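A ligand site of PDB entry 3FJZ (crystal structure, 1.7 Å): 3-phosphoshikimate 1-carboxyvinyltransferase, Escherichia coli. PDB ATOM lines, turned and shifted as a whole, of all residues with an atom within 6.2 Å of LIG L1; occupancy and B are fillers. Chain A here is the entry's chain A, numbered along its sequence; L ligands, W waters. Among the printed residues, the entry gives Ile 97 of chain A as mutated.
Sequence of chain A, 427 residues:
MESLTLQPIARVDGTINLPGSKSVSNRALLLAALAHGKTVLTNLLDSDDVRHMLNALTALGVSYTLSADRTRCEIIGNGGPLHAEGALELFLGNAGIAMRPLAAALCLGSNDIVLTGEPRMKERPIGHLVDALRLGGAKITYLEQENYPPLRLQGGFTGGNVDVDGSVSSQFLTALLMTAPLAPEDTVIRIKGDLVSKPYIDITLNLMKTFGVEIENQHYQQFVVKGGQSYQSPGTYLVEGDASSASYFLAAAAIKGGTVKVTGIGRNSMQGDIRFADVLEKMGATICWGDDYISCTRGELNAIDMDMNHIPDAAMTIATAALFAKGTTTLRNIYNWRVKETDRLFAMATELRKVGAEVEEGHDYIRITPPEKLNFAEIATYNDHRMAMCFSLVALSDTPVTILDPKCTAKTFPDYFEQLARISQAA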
ATOM      1  N   LYS A  22     -14.310   8.789  22.109  1.00  0.00           N
ATOM      2  CA  LYS A  22     -15.731   8.671  22.442  1.00  0.00           C
ATOM      3  C   LYS A  22     -16.078   7.202  22.737  1.00  0.00           C
ATOM      4  O   LYS A  22     -16.775   6.890  23.710  1.00  0.00           O
ATOM      5  CB  LYS A  22     -16.594   9.196  21.272  1.00  0.00           C
ATOM      6  CG  LYS A  22     -18.114   9.018  21.474  1.00  0.00           C
ATOM      7  CD  LYS A  22     -18.747   8.026  20.461  1.00  0.00           C
ATOM      8  CE  LYS A  22     -18.777   8.632  19.049  1.00  0.00           C
ATOM      9  NZ  LYS A  22     -19.122   7.610  17.988  1.00  0.00           N
ATOM     10  N   ASP A  49     -21.940  13.156  23.210  1.00  0.00           N
ATOM     11  CA  ASP A  49     -22.157  11.721  23.429  1.00  0.00           C
ATOM     12  C   ASP A  49     -21.778  11.282  24.832  1.00  0.00           C
ATOM     13  O   ASP A  49     -22.473  10.458  25.439  1.00  0.00           O
ATOM     14  CB  ASP A  49     -21.410  10.889  22.370  1.00  0.00           C
ATOM     15  CG  ASP A  49     -22.138  10.861  21.009  1.00  0.00           C
ATOM     16  OD1 ASP A  49     -23.203  11.511  20.853  1.00  0.00           O
ATOM     17  OD2 ASP A  49     -21.628  10.187  20.084  1.00  0.00           O
ATOM     18  N   ASN A  94     -28.073  11.597  20.223  1.00  0.00           N
ATOM     19  CA  ASN A  94     -27.986  10.686  19.085  1.00  0.00           C
ATOM     20  C   ASN A  94     -26.743   9.840  19.295  1.00  0.00           C
ATOM     21  O   ASN A  94     -26.038   9.465  18.361  1.00  0.00           O
ATOM     22  CB  ASN A  94     -27.904  11.467  17.758  1.00  0.00           C
ATOM     23  CG  ASN A  94     -28.139  10.565  16.535  1.00  0.00           C
ATOM     24  OD1 ASN A  94     -28.649   9.460  16.666  1.00  0.00           O
ATOM     25  ND2 ASN A  94     -27.801  11.067  15.348  1.00  0.00           N
ATOM     26  N   ALA A  95     -26.495   9.515  20.567  1.00  0.00           N
ATOM     27  CA  ALA A  95     -25.325   8.707  20.943  1.00  0.00           C
ATOM     28  C   ALA A  95     -25.574   7.202  20.874  1.00  0.00           C
ATOM     29  O   ALA A  95     -26.116   6.612  21.793  1.00  0.00           O
ATOM     30  CB  ALA A  95     -24.886   9.081  22.376  1.00  0.00           C
ATOM     31  N   GLY A  96     -25.194   6.595  19.759  1.00  0.00           N
ATOM     32  CA  GLY A  96     -25.389   5.160  19.646  1.00  0.00           C
ATOM     33  C   GLY A  96     -24.644   4.388  20.714  1.00  0.00           C
ATOM     34  O   GLY A  96     -25.160   3.391  21.227  1.00  0.00           O
ATOM     35  N   ILE A  97     -23.430   4.807  21.056  1.00  0.00           N
ATOM     36  CA  ILE A  97     -22.660   4.058  22.036  1.00  0.00           C
ATOM     37  C   ILE A  97     -23.120   4.320  23.472  1.00  0.00           C
ATOM     38  O   ILE A  97     -22.504   3.838  24.435  1.00  0.00           O
ATOM     39  CB  ILE A  97     -21.115   4.228  21.810  1.00  0.00           C
ATOM     40  CG1 ILE A  97     -20.347   3.021  22.419  1.00  0.00           C
ATOM     41  CG2 ILE A  97     -20.656   5.547  22.381  1.00  0.00           C
ATOM     42  CD1 ILE A  97     -20.697   1.658  21.799  1.00  0.00           C
ATOM     43  N   ARG A 100     -27.159   1.957  22.609  1.00  0.00           N
ATOM     44  CA  ARG A 100     -27.083   0.521  22.477  1.00  0.00           C
ATOM     45  C   ARG A 100     -26.610  -0.164  23.775  1.00  0.00           C
ATOM     46  O   ARG A 100     -27.289  -1.051  24.282  1.00  0.00           O
ATOM     47  CB  ARG A 100     -26.227   0.132  21.253  1.00  0.00           C
ATOM     48  CG  ARG A 100     -26.987   0.180  19.901  1.00  0.00           C
ATOM     49  CD  ARG A 100     -27.446   1.612  19.515  1.00  0.00           C
ATOM     50  NE  ARG A 100     -28.050   1.676  18.170  1.00  0.00           N
ATOM     51  CZ  ARG A 100     -27.357   1.841  17.040  1.00  0.00           C
ATOM     52  NH1 ARG A 100     -27.983   1.897  15.878  1.00  0.00           N
ATOM     53  NH2 ARG A 100     -26.015   1.983  17.054  1.00  0.00           N
ATOM     54  N   MET A 121     -32.285   9.725  16.194  1.00  0.00           N
ATOM     55  CA  MET A 121     -32.059   8.478  16.944  1.00  0.00           C
ATOM     56  C   MET A 121     -33.279   7.575  16.845  1.00  0.00           C
ATOM     57  O   MET A 121     -33.137   6.333  16.871  1.00  0.00           O
ATOM     58  CB  MET A 121     -31.714   8.772  18.418  1.00  0.00           C
ATOM     59  CG  MET A 121     -31.550   7.520  19.306  1.00  0.00           C
ATOM     60  SD  MET A 121     -30.331   6.299  18.682  1.00  0.00           S
ATOM     61  CE  MET A 121     -28.764   7.094  19.175  1.00  0.00           C
ATOM     62  N   ARG A 124     -32.762   5.335  13.896  1.00  0.00           N
ATOM     63  CA  ARG A 124     -31.577   4.484  13.792  1.00  0.00           C
ATOM     64  C   ARG A 124     -31.980   3.144  14.393  1.00  0.00           C
ATOM     65  O   ARG A 124     -32.453   3.064  15.530  1.00  0.00           O
ATOM     66  CB  ARG A 124     -30.402   5.118  14.525  1.00  0.00           C
ATOM     67  CG  ARG A 124     -29.936   6.412  13.808  1.00  0.00           C
ATOM     68  CD  ARG A 124     -28.721   7.018  14.489  1.00  0.00           C
ATOM     69  NE  ARG A 124     -27.610   6.082  14.462  1.00  0.00           N
ATOM     70  CZ  ARG A 124     -26.536   6.183  15.235  1.00  0.00           C
ATOM     71  NH1 ARG A 124     -25.569   5.268  15.124  1.00  0.00           N
ATOM     72  NH2 ARG A 124     -26.410   7.183  16.117  1.00  0.00           N
ATOM     73  N   GLN A 171     -22.406  -2.559  17.381  1.00  0.00           N
ATOM     74  CA  GLN A 171     -22.821  -2.096  18.694  1.00  0.00           C
ATOM     75  C   GLN A 171     -23.788  -3.012  19.410  1.00  0.00           C
ATOM     76  O   GLN A 171     -23.841  -3.024  20.641  1.00  0.00           O
ATOM     77  CB  GLN A 171     -23.421  -0.706  18.611  1.00  0.00           C
ATOM     78  CG  GLN A 171     -22.369   0.322  18.302  1.00  0.00           C
ATOM     79  CD  GLN A 171     -22.912   1.723  18.371  1.00  0.00           C
ATOM     80  OE1 GLN A 171     -23.981   1.961  18.923  1.00  0.00           O
ATOM     81  NE2 GLN A 171     -22.170   2.674  17.811  1.00  0.00           N
ATOM     82  N   ASP A 313     -15.914   5.130  10.203  1.00  0.00           N
ATOM     83  CA  ASP A 313     -15.962   6.537  10.593  1.00  0.00           C
ATOM     84  C   ASP A 313     -14.831   7.334   9.977  1.00  0.00           C
ATOM     85  O   ASP A 313     -15.065   8.332   9.297  1.00  0.00           O
ATOM     86  CB  ASP A 313     -15.898   6.672  12.109  1.00  0.00           C
ATOM     87  CG  ASP A 313     -17.132   6.134  12.811  1.00  0.00           C
ATOM     88  OD1 ASP A 313     -17.136   6.197  14.044  1.00  0.00           O
ATOM     89  OD2 ASP A 313     -18.081   5.667  12.140  1.00  0.00           O
ATOM     90  N   MET A 316     -14.806   8.346   6.189  1.00  0.00           N
ATOM     91  CA  MET A 316     -15.446   9.545   5.639  1.00  0.00           C
ATOM     92  C   MET A 316     -14.389  10.591   5.313  1.00  0.00           C
ATOM     93  O   MET A 316     -14.531  11.353   4.355  1.00  0.00           O
ATOM     94  CB  MET A 316     -16.432  10.144   6.630  1.00  0.00           C
ATOM     95  CG  MET A 316     -17.602   9.241   6.961  1.00  0.00           C
ATOM     96  SD  MET A 316     -18.681  10.047   8.148  1.00  0.00           S
ATOM     97  CE  MET A 316     -19.383  11.451   7.194  1.00  0.00           C
ATOM     98  N   LYS A 340     -26.325   5.873  10.324  1.00  0.00           N
ATOM     99  CA  LYS A 340     -25.663   6.581  11.412  1.00  0.00           C
ATOM    100  C   LYS A 340     -26.207   7.977  11.673  1.00  0.00           C
ATOM    101  O   LYS A 340     -27.414   8.175  11.574  1.00  0.00           O
ATOM    102  CB  LYS A 340     -24.166   6.541  11.202  1.00  0.00           C
ATOM    103  CG  LYS A 340     -23.672   5.122  11.571  1.00  0.00           C
ATOM    104  CD  LYS A 340     -22.271   4.826  11.132  1.00  0.00           C
ATOM    105  CE  LYS A 340     -21.896   3.432  11.640  1.00  0.00           C
ATOM    106  NZ  LYS A 340     -20.566   3.008  11.174  1.00  0.00           N
ATOM    107  N   GLU A 341     -25.367   8.960  12.005  1.00  0.00           N
ATOM    108  CA  GLU A 341     -25.873  10.291  12.334  1.00  0.00           C
ATOM    109  C   GLU A 341     -26.829  10.856  11.309  1.00  0.00           C
ATOM    110  O   GLU A 341     -27.742  11.613  11.632  1.00  0.00           O
ATOM    111  CB  GLU A 341     -24.720  11.264  12.609  1.00  0.00           C
ATOM    112  CG  GLU A 341     -24.087  11.050  14.012  1.00  0.00           C
ATOM    113  CD  GLU A 341     -23.054   9.931  14.097  1.00  0.00           C
ATOM    114  OE1 GLU A 341     -23.029   8.992  13.244  1.00  0.00           O
ATOM    115  OE2 GLU A 341     -22.253   9.978  15.064  1.00  0.00           O
ATOM    116  N   ARG A 344     -25.106   8.851   5.565  1.00  0.00           N
ATOM    117  CA  ARG A 344     -23.847   9.401   5.126  1.00  0.00           C
ATOM    118  C   ARG A 344     -23.501   9.167   3.675  1.00  0.00           C
ATOM    119  O   ARG A 344     -22.738   9.936   3.096  1.00  0.00           O
ATOM    120  CB  ARG A 344     -22.730   8.907   6.050  1.00  0.00           C
ATOM    121  CG  ARG A 344     -22.818   9.571   7.431  1.00  0.00           C
ATOM    122  CD  ARG A 344     -21.893   8.901   8.423  1.00  0.00           C
ATOM    123  NE  ARG A 344     -21.645   9.817   9.539  1.00  0.00           N
ATOM    124  CZ  ARG A 344     -20.951   9.492  10.619  1.00  0.00           C
ATOM    125  NH1 ARG A 344     -20.753  10.397  11.591  1.00  0.00           N
ATOM    126  NH2 ARG A 344     -20.455   8.261  10.728  1.00  0.00           N
ATOM    127  N   ASP A 384     -24.563  16.159  11.646  1.00  0.00           N
ATOM    128  CA  ASP A 384     -23.513  15.149  11.669  1.00  0.00           C
ATOM    129  C   ASP A 384     -22.131  15.758  11.842  1.00  0.00           C
ATOM    130  O   ASP A 384     -21.586  16.347  10.893  1.00  0.00           O
ATOM    131  CB  ASP A 384     -23.561  14.352  10.363  1.00  0.00           C
ATOM    132  CG  ASP A 384     -22.607  13.166  10.352  1.00  0.00           C
ATOM    133  OD1 ASP A 384     -21.764  13.078  11.271  1.00  0.00           O
ATOM    134  OD2 ASP A 384     -22.686  12.339   9.399  1.00  0.00           O
ATOM    135  N   HIS A 385     -21.584  15.616  13.043  1.00  0.00           N
ATOM    136  CA  HIS A 385     -20.248  16.121  13.347  1.00  0.00           C
ATOM    137  C   HIS A 385     -19.240  15.819  12.248  1.00  0.00           C
ATOM    138  O   HIS A 385     -18.442  16.701  11.890  1.00  0.00           O
ATOM    139  CB  HIS A 385     -19.739  15.550  14.689  1.00  0.00           C
ATOM    140  CG  HIS A 385     -19.781  14.045  14.756  1.00  0.00           C
ATOM    141  ND1 HIS A 385     -18.762  13.311  15.330  1.00  0.00           N
ATOM    142  CD2 HIS A 385     -20.724  13.148  14.374  1.00  0.00           C
ATOM    143  CE1 HIS A 385     -19.081  12.030  15.313  1.00  0.00           C
ATOM    144  NE2 HIS A 385     -20.266  11.895  14.734  1.00  0.00           N
ATOM    145  N   ARG A 386     -19.272  14.609  11.674  1.00  0.00           N
ATOM    146  CA  ARG A 386     -18.268  14.287  10.672  1.00  0.00           C
ATOM    147  C   ARG A 386     -18.461  14.970   9.333  1.00  0.00           C
ATOM    148  O   ARG A 386     -17.494  15.129   8.591  1.00  0.00           O
ATOM    149  CB  ARG A 386     -18.121  12.767  10.523  1.00  0.00           C
ATOM    150  CG  ARG A 386     -17.699  12.105  11.843  1.00  0.00           C
ATOM    151  CD  ARG A 386     -16.930  10.777  11.652  1.00  0.00           C
ATOM    152  NE  ARG A 386     -16.836  10.149  12.977  1.00  0.00           N
ATOM    153  CZ  ARG A 386     -16.018  10.533  13.952  1.00  0.00           C
ATOM    154  NH1 ARG A 386     -16.094   9.905  15.134  1.00  0.00           N
ATOM    155  NH2 ARG A 386     -15.084  11.467  13.745  1.00  0.00           N
ATOM    156  N   LYS A 411     -20.741  16.752  18.908  1.00  0.00           N
ATOM    157  CA  LYS A 411     -21.111  15.376  19.232  1.00  0.00           C
ATOM    158  C   LYS A 411     -19.884  14.611  19.762  1.00  0.00           C
ATOM    159  O   LYS A 411     -19.981  13.841  20.722  1.00  0.00           O
ATOM    160  CB  LYS A 411     -21.670  14.615  18.018  1.00  0.00           C
ATOM    161  CG  LYS A 411     -22.360  13.309  18.410  1.00  0.00           C
ATOM    162  CD  LYS A 411     -23.171  12.741  17.236  1.00  0.00           C
ATOM    163  CE  LYS A 411     -23.985  11.524  17.654  1.00  0.00           C
ATOM    164  NZ  LYS A 411     -23.134  10.298  17.762  1.00  0.00           N
ATOM    165  N   THR A 412     -18.736  14.853  19.145  1.00  0.00           N
ATOM    166  CA  THR A 412     -17.503  14.198  19.569  1.00  0.00           C
ATOM    167  C   THR A 412     -16.293  15.106  19.678  1.00  0.00           C
ATOM    168  O   THR A 412     -15.268  14.690  20.202  1.00  0.00           O
ATOM    169  CB  THR A 412     -17.067  13.106  18.573  1.00  0.00           C
ATOM    170  OG1 THR A 412     -16.813  13.695  17.278  1.00  0.00           O
ATOM    171  CG2 THR A 412     -18.099  12.013  18.477  1.00  0.00           C
HETATM  172  C1  LIG L   1     -22.446   6.526  15.430  1.00  0.00           C
HETATM  173  C2  LIG L   1     -20.623   7.500  13.999  1.00  0.00           C
HETATM  174  C3  LIG L   1     -19.397   8.398  14.119  1.00  0.00           C
HETATM  175  O1  LIG L   1     -21.680   6.431  17.929  1.00  0.00           O
HETATM  176  O2  LIG L   1     -23.573   4.991  17.091  1.00  0.00           O
HETATM  177  O3  LIG L   1     -23.860   7.469  17.438  1.00  0.00           O
HETATM  178  O4  LIG L   1     -19.022   8.773  15.284  1.00  0.00           O
HETATM  179  P1  LIG L   1     -22.903   6.334  17.088  1.00  0.00           P
HETATM  180  O5  LIG L   1     -18.838   8.710  13.069  1.00  0.00           O
HETATM  181  N1  LIG L   1     -21.188   7.245  15.317  1.00  0.00           N
HETATM  182  C1  LG2 L   2     -18.656   2.448  17.664  1.00  0.00           C
HETATM  183  C2  LG2 L   2     -18.906   1.546  16.604  1.00  0.00           C
HETATM  184  C3  LG2 L   2     -19.269   2.038  15.218  1.00  0.00           C
HETATM  185  C4  LG2 L   2     -18.885   3.532  15.013  1.00  0.00           C
HETATM  186  C5  LG2 L   2     -19.330   4.404  16.193  1.00  0.00           C
HETATM  187  C6  LG2 L   2     -18.681   3.876  17.477  1.00  0.00           C
HETATM  188  C7  LG2 L   2     -18.311   1.885  19.021  1.00  0.00           C
HETATM  189  O1  LG2 L   2     -20.700   1.728  14.907  1.00  0.00           O
HETATM  190  O2  LG2 L   2     -19.436   3.966  13.769  1.00  0.00           O
HETATM  191  O3  LG2 L   2     -18.937   5.762  15.983  1.00  0.00           O
HETATM  192  O4  LG2 L   2     -18.572   0.679  19.229  1.00  0.00           O
HETATM  193  O5  LG2 L   2     -17.712   2.610  19.788  1.00  0.00           O
HETATM  194  P1  LG2 L   2     -21.239   0.439  13.922  1.00  0.00           P
HETATM  195  O6  LG2 L   2     -20.871  -0.848  14.567  1.00  0.00           O
HETATM  196  O7  LG2 L   2     -20.540   0.590  12.596  1.00  0.00           O
HETATM  197  O8  LG2 L   2     -22.703   0.550  13.822  1.00  0.00           O
HETATM  198  O   HOH W   1     -23.902   2.771  15.030  1.00  0.00           O
HETATM  199  O   HOH W   2     -22.115   7.390  20.277  1.00  0.00           O
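NH1 of Arg 124 is in salt-bridge range of O2 of LIG L1 (2.8 Å).
The side-chain amino group of Lys 22 lies within salt-bridge range of an oxygen (O1) of LIG L1, at 2.8 Å.
NH2 of Arg 100 lies within salt-bridge range of O2 of LIG L1 (3.9 Å).
The backbone carbonyl oxygen (O) of Asn 94 sits close to an oxygen (O3) of LIG L1 (3.1 Å).
The guanidinium group of Arg 344 is in salt-bridge range of an oxygen (O5) of LIG L1, at 2.9 Å.
An oxygen (O3) of LG2 L2 sits at hydrogen-bond distance from the side-chain carboxylate (OD1) of Asp 313 (2.7 Å).
The side-chain carboxylate (OE2) of Glu 341 lies within salt-bridge range of a nitrogen (N1) of LIG L1 (2.9 Å).
An oxygen (O2) of LIG L1 lies within hydrogen-bond range of the side-chain amide nitrogen of Gln 171.
NZ of Lys 411 is in salt-bridge range of O3 of LIG L1, 2.9 Å away.
An oxygen (O3) of LIG L1 is in hydrogen-bond range of the backbone NH (N) of Gly 96 (2.8 Å).
The side-chain amino group (NZ) of Lys 340 is in salt-bridge range of an oxygen (O7) of LG2 L2 (2.8 Å).
NE of Arg 386 lies within salt-bridge range of O5 of LIG L1 (2.5 Å).
An oxygen (O1) of LG2 L2 lies within hydrogen-bond range of the side-chain amide nitrogen of Gln 171 (3.4 Å).
The side-chain amino group (NZ) of Lys 22 sits at hydrogen-bond distance from an oxygen (O3) of LG2 L2.
NE2 of His 385 lies close to O4 of LIG L1 (3.4 Å).
The side-chain carboxylate (OD1) of Asp 313 sits close to an oxygen (O5) of LIG L1.
Merely in contact with LIG L1: Ala 95 (3.8 Å) and Ile 97 (3.9 Å).
Hydrophobic or aromatic side chains that line LIG L1: His 385.
The nearest printed residue that does not touch LIG L1 is Lys 340 (4.3 Å).
A ring nitrogen (NE2) of His 385 lies within hydrogen-bond range of the side-chain carboxylate of Glu 341 (2.8 Å).
OE2 of Glu 341 is in salt-bridge range of NZ of Lys 411 (2.9 Å).
OE1 of Gln 171 sits close to O of Gly 96.
OG1 of Thr 412 sits at hydrogen-bond distance from ND1 of His 385 (2.8 Å).
The side-chain sulfur of Met 316 is in hydrogen-bond range of the guanidinium group of Arg 344 (3.3 Å).
The side-chain amino group of Lys 411 lies within salt-bridge range of the side-chain carboxylate of Asp 49 (2.8 Å).
The side-chain amide oxygen (OE1) of Gln 171 lies within hydrogen-bond range of the guanidinium group (NH2) of Arg 100, at 2.8 Å.
O of Asn 94 lies within hydrogen-bond range of NH2 of Arg 124, 3.2 Å away.
A nitrogen (N1) of LIG L1 sits at hydrogen-bond distance from an oxygen (O3) of LG2 L2 (2.8 Å).
Water W2 lies within hydrogen-bond range of O1 of LIG L1, OD2 of Asp 49, N of Ile 97 and N of Gly 96.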
